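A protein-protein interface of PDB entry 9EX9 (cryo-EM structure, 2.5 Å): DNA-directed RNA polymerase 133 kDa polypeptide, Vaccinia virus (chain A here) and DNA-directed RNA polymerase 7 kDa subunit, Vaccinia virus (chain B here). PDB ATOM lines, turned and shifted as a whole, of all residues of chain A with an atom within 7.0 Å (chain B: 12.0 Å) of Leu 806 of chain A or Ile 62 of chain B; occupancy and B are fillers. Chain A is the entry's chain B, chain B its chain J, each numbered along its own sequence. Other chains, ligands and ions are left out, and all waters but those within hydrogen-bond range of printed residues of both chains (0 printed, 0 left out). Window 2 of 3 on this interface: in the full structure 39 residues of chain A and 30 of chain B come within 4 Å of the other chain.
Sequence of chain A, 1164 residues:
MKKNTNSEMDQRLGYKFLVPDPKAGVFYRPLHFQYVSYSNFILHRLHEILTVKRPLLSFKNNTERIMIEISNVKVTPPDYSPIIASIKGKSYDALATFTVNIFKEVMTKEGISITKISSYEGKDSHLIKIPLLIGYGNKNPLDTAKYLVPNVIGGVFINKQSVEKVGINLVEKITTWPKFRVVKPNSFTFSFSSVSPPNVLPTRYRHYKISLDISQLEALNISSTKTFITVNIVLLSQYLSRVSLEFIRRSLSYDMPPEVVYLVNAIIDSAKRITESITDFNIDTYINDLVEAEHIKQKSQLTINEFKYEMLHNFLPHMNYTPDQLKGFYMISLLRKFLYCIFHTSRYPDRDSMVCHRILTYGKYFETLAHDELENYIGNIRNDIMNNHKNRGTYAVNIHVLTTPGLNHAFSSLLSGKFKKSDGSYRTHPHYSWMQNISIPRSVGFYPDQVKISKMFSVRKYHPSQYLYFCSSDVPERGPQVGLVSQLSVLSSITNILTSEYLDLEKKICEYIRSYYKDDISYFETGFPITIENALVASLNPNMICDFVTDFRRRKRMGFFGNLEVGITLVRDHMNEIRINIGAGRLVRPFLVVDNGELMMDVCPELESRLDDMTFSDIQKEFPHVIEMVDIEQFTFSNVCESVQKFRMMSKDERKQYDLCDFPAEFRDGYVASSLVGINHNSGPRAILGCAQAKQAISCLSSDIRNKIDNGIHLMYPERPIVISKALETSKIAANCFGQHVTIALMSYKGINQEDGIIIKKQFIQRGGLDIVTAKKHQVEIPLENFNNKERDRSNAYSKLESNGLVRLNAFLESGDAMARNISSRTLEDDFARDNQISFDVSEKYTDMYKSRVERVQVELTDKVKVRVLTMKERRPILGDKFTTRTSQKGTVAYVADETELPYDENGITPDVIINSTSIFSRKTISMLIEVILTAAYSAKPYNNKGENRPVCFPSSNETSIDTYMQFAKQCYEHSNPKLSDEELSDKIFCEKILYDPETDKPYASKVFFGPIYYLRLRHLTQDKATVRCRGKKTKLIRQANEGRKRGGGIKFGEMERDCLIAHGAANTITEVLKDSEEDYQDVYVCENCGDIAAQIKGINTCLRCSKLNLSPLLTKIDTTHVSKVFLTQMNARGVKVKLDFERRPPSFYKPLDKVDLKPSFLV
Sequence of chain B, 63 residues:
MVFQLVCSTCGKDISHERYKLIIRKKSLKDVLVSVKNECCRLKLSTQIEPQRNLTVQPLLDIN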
ATOM      1  N   LYS A  88     -19.496  16.078 -25.506  1.00  0.00           N
ATOM      2  CA  LYS A  88     -20.205  14.980 -24.864  1.00  0.00           C
ATOM      3  C   LYS A  88     -19.299  13.797 -24.568  1.00  0.00           C
ATOM      4  O   LYS A  88     -19.557  13.061 -23.612  1.00  0.00           O
ATOM      5  CB  LYS A  88     -21.361  14.514 -25.744  1.00  0.00           C
ATOM      6  CG  LYS A  88     -22.386  15.580 -26.045  1.00  0.00           C
ATOM      7  CD  LYS A  88     -23.151  15.978 -24.808  1.00  0.00           C
ATOM      8  CE  LYS A  88     -24.239  16.978 -25.135  1.00  0.00           C
ATOM      9  NZ  LYS A  88     -24.949  17.446 -23.915  1.00  0.00           N
ATOM     10  N   ILE A 782     -16.021   7.160 -11.343  1.00  0.00           N
ATOM     11  CA  ILE A 782     -16.388   6.969  -9.943  1.00  0.00           C
ATOM     12  C   ILE A 782     -17.533   5.964  -9.846  1.00  0.00           C
ATOM     13  O   ILE A 782     -18.543   6.112 -10.549  1.00  0.00           O
ATOM     14  CB  ILE A 782     -16.778   8.309  -9.302  1.00  0.00           C
ATOM     15  CG1 ILE A 782     -15.607   9.288  -9.392  1.00  0.00           C
ATOM     16  CG2 ILE A 782     -17.200   8.113  -7.859  1.00  0.00           C
ATOM     17  CD1 ILE A 782     -15.926  10.667  -8.889  1.00  0.00           C
ATOM     18  N   PHE A 787     -19.886   8.140  -5.321  1.00  0.00           N
ATOM     19  CA  PHE A 787     -20.293   9.490  -5.692  1.00  0.00           C
ATOM     20  C   PHE A 787     -21.450   9.972  -4.828  1.00  0.00           C
ATOM     21  O   PHE A 787     -21.491  11.140  -4.427  1.00  0.00           O
ATOM     22  CB  PHE A 787     -20.671   9.530  -7.170  1.00  0.00           C
ATOM     23  CG  PHE A 787     -21.052  10.892  -7.660  1.00  0.00           C
ATOM     24  CD1 PHE A 787     -20.109  11.900  -7.745  1.00  0.00           C
ATOM     25  CD2 PHE A 787     -22.350  11.162  -8.047  1.00  0.00           C
ATOM     26  CE1 PHE A 787     -20.457  13.151  -8.199  1.00  0.00           C
ATOM     27  CE2 PHE A 787     -22.701  12.413  -8.503  1.00  0.00           C
ATOM     28  CZ  PHE A 787     -21.753  13.408  -8.579  1.00  0.00           C
ATOM     29  N   LYS A 800     -13.293  22.894  -2.424  1.00  0.00           N
ATOM     30  CA  LYS A 800     -13.759  23.500  -3.662  1.00  0.00           C
ATOM     31  C   LYS A 800     -15.002  22.821  -4.221  1.00  0.00           C
ATOM     32  O   LYS A 800     -15.396  23.115  -5.352  1.00  0.00           O
ATOM     33  CB  LYS A 800     -12.646  23.472  -4.712  1.00  0.00           C
ATOM     34  CG  LYS A 800     -11.308  24.009  -4.233  1.00  0.00           C
ATOM     35  CD  LYS A 800     -11.345  25.506  -4.011  1.00  0.00           C
ATOM     36  CE  LYS A 800     -10.108  25.981  -3.271  1.00  0.00           C
ATOM     37  NZ  LYS A 800      -8.852  25.561  -3.944  1.00  0.00           N
ATOM     38  N   LEU A 801     -15.627  21.925  -3.464  1.00  0.00           N
ATOM     39  CA  LEU A 801     -16.762  21.151  -3.941  1.00  0.00           C
ATOM     40  C   LEU A 801     -18.080  21.803  -3.549  1.00  0.00           C
ATOM     41  O   LEU A 801     -18.251  22.279  -2.425  1.00  0.00           O
ATOM     42  CB  LEU A 801     -16.715  19.727  -3.394  1.00  0.00           C
ATOM     43  CG  LEU A 801     -15.989  18.723  -4.281  1.00  0.00           C
ATOM     44  CD1 LEU A 801     -14.614  19.229  -4.638  1.00  0.00           C
ATOM     45  CD2 LEU A 801     -15.897  17.385  -3.588  1.00  0.00           C
ATOM     46  N   GLU A 802     -19.016  21.808  -4.492  1.00  0.00           N
ATOM     47  CA  GLU A 802     -20.354  22.320  -4.259  1.00  0.00           C
ATOM     48  C   GLU A 802     -21.197  21.266  -3.545  1.00  0.00           C
ATOM     49  O   GLU A 802     -20.733  20.169  -3.228  1.00  0.00           O
ATOM     50  CB  GLU A 802     -20.997  22.733  -5.578  1.00  0.00           C
ATOM     51  CG  GLU A 802     -20.496  24.049  -6.122  1.00  0.00           C
ATOM     52  CD  GLU A 802     -20.997  25.233  -5.324  1.00  0.00           C
ATOM     53  OE1 GLU A 802     -21.732  25.015  -4.340  1.00  0.00           O
ATOM     54  OE2 GLU A 802     -20.663  26.381  -5.681  1.00  0.00           O
ATOM     55  N   SER A 803     -22.461  21.600  -3.288  1.00  0.00           N
ATOM     56  CA  SER A 803     -23.342  20.673  -2.590  1.00  0.00           C
ATOM     57  C   SER A 803     -23.626  19.417  -3.401  1.00  0.00           C
ATOM     58  O   SER A 803     -24.047  18.410  -2.825  1.00  0.00           O
ATOM     59  CB  SER A 803     -24.659  21.360  -2.236  1.00  0.00           C
ATOM     60  OG  SER A 803     -25.402  21.663  -3.402  1.00  0.00           O
ATOM     61  N   ASN A 804     -23.411  19.448  -4.712  1.00  0.00           N
ATOM     62  CA  ASN A 804     -23.696  18.308  -5.570  1.00  0.00           C
ATOM     63  C   ASN A 804     -22.486  17.408  -5.776  1.00  0.00           C
ATOM     64  O   ASN A 804     -22.545  16.495  -6.604  1.00  0.00           O
ATOM     65  CB  ASN A 804     -24.230  18.783  -6.925  1.00  0.00           C
ATOM     66  CG  ASN A 804     -23.192  19.522  -7.745  1.00  0.00           C
ATOM     67  OD1 ASN A 804     -22.006  19.516  -7.427  1.00  0.00           O
ATOM     68  ND2 ASN A 804     -23.638  20.163  -8.816  1.00  0.00           N
ATOM     69  N   GLY A 805     -21.396  17.641  -5.053  1.00  0.00           N
ATOM     70  CA  GLY A 805     -20.234  16.787  -5.160  1.00  0.00           C
ATOM     71  C   GLY A 805     -19.329  17.083  -6.331  1.00  0.00           C
ATOM     72  O   GLY A 805     -18.417  16.294  -6.600  1.00  0.00           O
ATOM     73  N   LEU A 806     -19.549  18.189  -7.035  1.00  0.00           N
ATOM     74  CA  LEU A 806     -18.737  18.580  -8.174  1.00  0.00           C
ATOM     75  C   LEU A 806     -18.047  19.905  -7.884  1.00  0.00           C
ATOM     76  O   LEU A 806     -18.579  20.755  -7.165  1.00  0.00           O
ATOM     77  CB  LEU A 806     -19.584  18.708  -9.444  1.00  0.00           C
ATOM     78  CG  LEU A 806     -20.257  17.431  -9.941  1.00  0.00           C
ATOM     79  CD1 LEU A 806     -21.209  17.749 -11.071  1.00  0.00           C
ATOM     80  CD2 LEU A 806     -19.224  16.422 -10.390  1.00  0.00           C
ATOM     81  N   VAL A 807     -16.856  20.072  -8.459  1.00  0.00           N
ATOM     82  CA  VAL A 807     -16.083  21.283  -8.228  1.00  0.00           C
ATOM     83  C   VAL A 807     -16.838  22.500  -8.751  1.00  0.00           C
ATOM     84  O   VAL A 807     -17.661  22.407  -9.669  1.00  0.00           O
ATOM     85  CB  VAL A 807     -14.698  21.164  -8.885  1.00  0.00           C
ATOM     86  CG1 VAL A 807     -14.831  21.015 -10.385  1.00  0.00           C
ATOM     87  CG2 VAL A 807     -13.842  22.363  -8.541  1.00  0.00           C
ATOM     88  N   ARG A 808     -16.553  23.653  -8.158  1.00  0.00           N
ATOM     89  CA  ARG A 808     -17.258  24.882  -8.484  1.00  0.00           C
ATOM     90  C   ARG A 808     -16.613  25.583  -9.676  1.00  0.00           C
ATOM     91  O   ARG A 808     -15.394  25.562  -9.852  1.00  0.00           O
ATOM     92  CB  ARG A 808     -17.268  25.810  -7.270  1.00  0.00           C
ATOM     93  CG  ARG A 808     -17.901  27.162  -7.512  1.00  0.00           C
ATOM     94  CD  ARG A 808     -17.949  27.993  -6.242  1.00  0.00           C
ATOM     95  NE  ARG A 808     -16.657  28.051  -5.567  1.00  0.00           N
ATOM     96  CZ  ARG A 808     -16.276  27.239  -4.589  1.00  0.00           C
ATOM     97  NH1 ARG A 808     -17.062  26.275  -4.141  1.00  0.00           N
ATOM     98  NH2 ARG A 808     -15.073  27.398  -4.046  1.00  0.00           N
ATOM     99  N   LEU A 809     -17.450  26.209 -10.498  1.00  0.00           N
ATOM    100  CA  LEU A 809     -16.951  26.939 -11.655  1.00  0.00           C
ATOM    101  C   LEU A 809     -16.119  28.138 -11.222  1.00  0.00           C
ATOM    102  O   LEU A 809     -16.456  28.835 -10.263  1.00  0.00           O
ATOM    103  CB  LEU A 809     -18.110  27.418 -12.529  1.00  0.00           C
ATOM    104  CG  LEU A 809     -18.840  26.404 -13.409  1.00  0.00           C
ATOM    105  CD1 LEU A 809     -19.900  27.114 -14.218  1.00  0.00           C
ATOM    106  CD2 LEU A 809     -17.883  25.676 -14.327  1.00  0.00           C
ATOM    107  N   ALA A 818      -9.486  17.775  -4.820  1.00  0.00           N
ATOM    108  CA  ALA A 818     -10.190  16.783  -5.614  1.00  0.00           C
ATOM    109  C   ALA A 818     -11.334  17.446  -6.369  1.00  0.00           C
ATOM    110  O   ALA A 818     -11.873  18.469  -5.939  1.00  0.00           O
ATOM    111  CB  ALA A 818     -10.735  15.658  -4.736  1.00  0.00           C
ATOM    112  N   MET A 819     -11.699  16.851  -7.501  1.00  0.00           N
ATOM    113  CA  MET A 819     -12.684  17.436  -8.400  1.00  0.00           C
ATOM    114  C   MET A 819     -14.081  16.858  -8.235  1.00  0.00           C
ATOM    115  O   MET A 819     -15.047  17.494  -8.669  1.00  0.00           O
ATOM    116  CB  MET A 819     -12.244  17.241  -9.853  1.00  0.00           C
ATOM    117  CG  MET A 819     -11.002  18.017 -10.240  1.00  0.00           C
ATOM    118  SD  MET A 819      -9.891  17.066 -11.292  1.00  0.00           S
ATOM    119  CE  MET A 819     -11.056  16.281 -12.403  1.00  0.00           C
ATOM    120  N   ALA A 820     -14.218  15.677  -7.638  1.00  0.00           N
ATOM    121  CA  ALA A 820     -15.525  15.067  -7.457  1.00  0.00           C
ATOM    122  C   ALA A 820     -15.488  14.151  -6.245  1.00  0.00           C
ATOM    123  O   ALA A 820     -14.492  13.470  -5.994  1.00  0.00           O
ATOM    124  CB  ALA A 820     -15.955  14.283  -8.699  1.00  0.00           C
ATOM    125  N   ARG A 821     -16.591  14.136  -5.501  1.00  0.00           N
ATOM    126  CA  ARG A 821     -16.649  13.374  -4.261  1.00  0.00           C
ATOM    127  C   ARG A 821     -16.613  11.880  -4.548  1.00  0.00           C
ATOM    128  O   ARG A 821     -17.364  11.378  -5.388  1.00  0.00           O
ATOM    129  CB  ARG A 821     -17.910  13.732  -3.480  1.00  0.00           C
ATOM    130  CG  ARG A 821     -18.030  13.004  -2.164  1.00  0.00           C
ATOM    131  CD  ARG A 821     -19.092  13.614  -1.276  1.00  0.00           C
ATOM    132  NE  ARG A 821     -20.392  13.674  -1.936  1.00  0.00           N
ATOM    133  CZ  ARG A 821     -21.105  14.776  -2.123  1.00  0.00           C
ATOM    134  NH1 ARG A 821     -20.695  15.955  -1.685  1.00  0.00           N
ATOM    135  NH2 ARG A 821     -22.268  14.693  -2.762  1.00  0.00           N
ATOM    136  N   VAL A 857     -16.975  21.927 -16.976  1.00  0.00           N
ATOM    137  CA  VAL A 857     -17.229  20.653 -16.305  1.00  0.00           C
ATOM    138  C   VAL A 857     -18.331  19.913 -17.052  1.00  0.00           C
ATOM    139  O   VAL A 857     -19.397  20.479 -17.311  1.00  0.00           O
ATOM    140  CB  VAL A 857     -17.634  20.853 -14.832  1.00  0.00           C
ATOM    141  CG1 VAL A 857     -17.919  19.517 -14.179  1.00  0.00           C
ATOM    142  CG2 VAL A 857     -16.552  21.594 -14.074  1.00  0.00           C
ATOM    143  N   GLN A 858     -18.084  18.642 -17.377  1.00  0.00           N
ATOM    144  CA  GLN A 858     -19.053  17.782 -18.045  1.00  0.00           C
ATOM    145  C   GLN A 858     -19.155  16.463 -17.295  1.00  0.00           C
ATOM    146  O   GLN A 858     -18.140  15.900 -16.873  1.00  0.00           O
ATOM    147  CB  GLN A 858     -18.656  17.517 -19.496  1.00  0.00           C
ATOM    148  CG  GLN A 858     -19.723  16.824 -20.317  1.00  0.00           C
ATOM    149  CD  GLN A 858     -20.832  17.759 -20.745  1.00  0.00           C
ATOM    150  OE1 GLN A 858     -20.661  18.975 -20.769  1.00  0.00           O
ATOM    151  NE2 GLN A 858     -21.980  17.193 -21.088  1.00  0.00           N
ATOM    152  N   VAL A 859     -20.379  15.966 -17.135  1.00  0.00           N
ATOM    153  CA  VAL A 859     -20.641  14.766 -16.349  1.00  0.00           C
ATOM    154  C   VAL A 859     -21.555  13.837 -17.132  1.00  0.00           C
ATOM    155  O   VAL A 859     -22.505  14.286 -17.783  1.00  0.00           O
ATOM    156  CB  VAL A 859     -21.271  15.109 -14.985  1.00  0.00           C
ATOM    157  CG1 VAL A 859     -21.487  13.850 -14.172  1.00  0.00           C
ATOM    158  CG2 VAL A 859     -20.391  16.083 -14.232  1.00  0.00           C
ATOM    159  N   GLU A 860     -21.268  12.540 -17.064  1.00  0.00           N
ATOM    160  CA  GLU A 860     -22.118  11.502 -17.630  1.00  0.00           C
ATOM    161  C   GLU A 860     -22.465  10.490 -16.549  1.00  0.00           C
ATOM    162  O   GLU A 860     -21.574   9.970 -15.869  1.00  0.00           O
ATOM    163  CB  GLU A 860     -21.436  10.805 -18.805  1.00  0.00           C
ATOM    164  CG  GLU A 860     -21.459  11.610 -20.086  1.00  0.00           C
ATOM    165  CD  GLU A 860     -22.868  11.837 -20.602  1.00  0.00           C
ATOM    166  OE1 GLU A 860     -23.806  11.218 -20.057  1.00  0.00           O
ATOM    167  OE2 GLU A 860     -23.037  12.635 -21.548  1.00  0.00           O
ATOM    168  N   LEU A 861     -23.757  10.212 -16.402  1.00  0.00           N
ATOM    169  CA  LEU A 861     -24.270   9.321 -15.369  1.00  0.00           C
ATOM    170  C   LEU A 861     -24.694   8.003 -16.004  1.00  0.00           C
ATOM    171  O   LEU A 861     -25.496   7.988 -16.944  1.00  0.00           O
ATOM    172  CB  LEU A 861     -25.448   9.959 -14.632  1.00  0.00           C
ATOM    173  CG  LEU A 861     -25.128  11.188 -13.785  1.00  0.00           C
ATOM    174  CD1 LEU A 861     -26.403  11.790 -13.226  1.00  0.00           C
ATOM    175  CD2 LEU A 861     -24.169  10.830 -12.662  1.00  0.00           C
ATOM    176  N   VAL A 865     -20.010   6.927 -12.919  1.00  0.00           N
ATOM    177  CA  VAL A 865     -20.060   8.367 -13.129  1.00  0.00           C
ATOM    178  C   VAL A 865     -18.756   8.781 -13.787  1.00  0.00           C
ATOM    179  O   VAL A 865     -17.676   8.454 -13.286  1.00  0.00           O
ATOM    180  CB  VAL A 865     -20.268   9.123 -11.805  1.00  0.00           C
ATOM    181  CG1 VAL A 865     -20.307  10.616 -12.048  1.00  0.00           C
ATOM    182  CG2 VAL A 865     -21.538   8.661 -11.126  1.00  0.00           C
ATOM    183  N   VAL A 867     -16.532  12.041 -15.118  1.00  0.00           N
ATOM    184  CA  VAL A 867     -16.387  13.481 -14.944  1.00  0.00           C
ATOM    185  C   VAL A 867     -15.193  13.953 -15.757  1.00  0.00           C
ATOM    186  O   VAL A 867     -14.113  13.354 -15.686  1.00  0.00           O
ATOM    187  CB  VAL A 867     -16.217  13.863 -13.463  1.00  0.00           C
ATOM    188  CG1 VAL A 867     -16.102  15.366 -13.316  1.00  0.00           C
ATOM    189  CG2 VAL A 867     -17.376  13.336 -12.638  1.00  0.00           C
ATOM    190  N   VAL B  56     -20.476  27.326 -26.129  1.00  0.00           N
ATOM    191  CA  VAL B  56     -21.572  26.405 -25.861  1.00  0.00           C
ATOM    192  C   VAL B  56     -21.990  26.547 -24.406  1.00  0.00           C
ATOM    193  O   VAL B  56     -21.153  26.479 -23.500  1.00  0.00           O
ATOM    194  CB  VAL B  56     -21.155  24.962 -26.176  1.00  0.00           C
ATOM    195  CG1 VAL B  56     -22.221  23.994 -25.710  1.00  0.00           C
ATOM    196  CG2 VAL B  56     -20.891  24.803 -27.659  1.00  0.00           C
ATOM    197  N   GLN B  57     -23.289  26.730 -24.178  1.00  0.00           N
ATOM    198  CA  GLN B  57     -23.836  26.902 -22.844  1.00  0.00           C
ATOM    199  C   GLN B  57     -24.865  25.815 -22.557  1.00  0.00           C
ATOM    200  O   GLN B  57     -25.551  25.354 -23.474  1.00  0.00           O
ATOM    201  CB  GLN B  57     -24.493  28.279 -22.701  1.00  0.00           C
ATOM    202  CG  GLN B  57     -23.556  29.431 -23.010  1.00  0.00           C
ATOM    203  CD  GLN B  57     -24.289  30.721 -23.290  1.00  0.00           C
ATOM    204  OE1 GLN B  57     -25.339  30.990 -22.713  1.00  0.00           O
ATOM    205  NE2 GLN B  57     -23.743  31.524 -24.190  1.00  0.00           N
ATOM    206  N   PRO B  58     -25.011  25.388 -21.294  1.00  0.00           N
ATOM    207  CA  PRO B  58     -24.347  25.859 -20.069  1.00  0.00           C
ATOM    208  C   PRO B  58     -22.904  25.402 -19.954  1.00  0.00           C
ATOM    209  O   PRO B  58     -22.479  24.477 -20.633  1.00  0.00           O
ATOM    210  CB  PRO B  58     -25.202  25.245 -18.944  1.00  0.00           C
ATOM    211  CG  PRO B  58     -26.406  24.629 -19.605  1.00  0.00           C
ATOM    212  CD  PRO B  58     -25.967  24.314 -20.994  1.00  0.00           C
ATOM    213  N   LEU B  59     -22.125  26.055 -19.093  1.00  0.00           N
ATOM    214  CA  LEU B  59     -20.746  25.645 -18.868  1.00  0.00           C
ATOM    215  C   LEU B  59     -20.651  24.450 -17.931  1.00  0.00           C
ATOM    216  O   LEU B  59     -19.640  23.741 -17.939  1.00  0.00           O
ATOM    217  CB  LEU B  59     -19.943  26.823 -18.318  1.00  0.00           C
ATOM    218  CG  LEU B  59     -19.752  27.976 -19.306  1.00  0.00           C
ATOM    219  CD1 LEU B  59     -19.416  29.263 -18.587  1.00  0.00           C
ATOM    220  CD2 LEU B  59     -18.664  27.638 -20.299  1.00  0.00           C
ATOM    221  N   LEU B  60     -21.677  24.215 -17.119  1.00  0.00           N
ATOM    222  CA  LEU B  60     -21.767  23.040 -16.258  1.00  0.00           C
ATOM    223  C   LEU B  60     -23.002  22.260 -16.685  1.00  0.00           C
ATOM    224  O   LEU B  60     -24.127  22.753 -16.552  1.00  0.00           O
ATOM    225  CB  LEU B  60     -21.848  23.445 -14.788  1.00  0.00           C
ATOM    226  CG  LEU B  60     -21.550  22.364 -13.748  1.00  0.00           C
ATOM    227  CD1 LEU B  60     -21.498  22.979 -12.369  1.00  0.00           C
ATOM    228  CD2 LEU B  60     -22.580  21.260 -13.782  1.00  0.00           C
ATOM    229  N   ASP B  61     -22.798  21.048 -17.194  1.00  0.00           N
ATOM    230  CA  ASP B  61     -23.883  20.247 -17.744  1.00  0.00           C
ATOM    231  C   ASP B  61     -23.849  18.850 -17.146  1.00  0.00           C
ATOM    232  O   ASP B  61     -22.795  18.209 -17.117  1.00  0.00           O
ATOM    233  CB  ASP B  61     -23.784  20.168 -19.268  1.00  0.00           C
ATOM    234  CG  ASP B  61     -25.053  19.645 -19.906  1.00  0.00           C
ATOM    235  OD1 ASP B  61     -26.123  20.249 -19.681  1.00  0.00           O
ATOM    236  OD2 ASP B  61     -24.980  18.639 -20.644  1.00  0.00           O
ATOM    237  N   ILE B  62     -25.003  18.385 -16.678  1.00  0.00           N
ATOM    238  CA  ILE B  62     -25.137  17.036 -16.143  1.00  0.00           C
ATOM    239  C   ILE B  62     -26.289  16.330 -16.847  1.00  0.00           C
ATOM    240  O   ILE B  62     -26.088  15.327 -17.533  1.00  0.00           O
ATOM    241  CB  ILE B  62     -25.360  17.046 -14.623  1.00  0.00           C
ATOM    242  CG1 ILE B  62     -24.325  17.939 -13.936  1.00  0.00           C
ATOM    243  CG2 ILE B  62     -25.270  15.635 -14.070  1.00  0.00           C
ATOM    244  CD1 ILE B  62     -24.499  18.033 -12.438  1.00  0.00           C
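The side-chain carboxylate (OD2) of Asp 61 of chain B lies within salt-bridge range of the side-chain amino group (NZ) of Lys 88 of chain A (3.5 Å).
N of Val 857 of chain A lies within hydrogen-bond range of O of Leu 59 of chain B (3.4 Å).
The side-chain carboxylate of Asp 61 of chain B lies within hydrogen-bond range of the side-chain amide nitrogen of Gln 858 of chain A (3.4 Å).
The backbone NH of Asp 61 of chain B is in hydrogen-bond range of the backbone carbonyl oxygen of Val 857 of chain A (3.5 Å).
N of Val 859 of chain A lies within hydrogen-bond range of O of Asp 61 of chain B, at 3.3 Å.
N of Leu 806 of chain A lies within hydrogen-bond range of OD1 of Asn 804 of chain A.
Among the printed residues, pairs that only touch across the chains: Leu 806 of chain A with Ile 62 of chain B, Val 857 of chain A with Leu 60 of chain B and Val 859 of chain A with Ile 62 of chain B.
Leu 806 of chain A touches just one residue of chain B: Ile 62.
Ile 62 of chain B touches just these residues of chain A: Leu 806 and Val 859.
No residue of chain B comes within 4 Å of Glu 802 of chain A.
No residue of chain B comes within 4 Å of Ser 803 of chain A.
No residue of chain B comes within 4 Å of Ala 820 of chain A.
Of the printed residues of chain B, Val 857 of chain A touches Leu 59, Leu 60 and Asp 61.
Of the printed residues of chain A, Asp 61 of chain B touches Lys 88, Val 857, Gln 858 and Val 859.
Of the printed residues of chain A, Leu 60 of chain B touches Val 857.
Of the printed residues of chain B, Lys 88 of chain A touches Asp 61 (3.5 Å).
Met 819 of chain A touches none of the printed residues of chain B.
The nearest residue of chain B that does not touch Leu 806 of chain A is Leu 60 of chain B (4.6 Å).
The nearest residue of chain A that does not touch Ile 62 of chain B is Leu 861 of chain A (4.1 Å).
Of the 24 printed residues of chain A, 5 touch a printed residue of chain B.
Printed residues of chain A that touch a printed residue of chain B: Lys 88, Leu 806, Val 857, Gln 858 and Val 859.
Hydrophobic or aromatic side chains of chain A that line the printed part of chain B: Leu 806.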
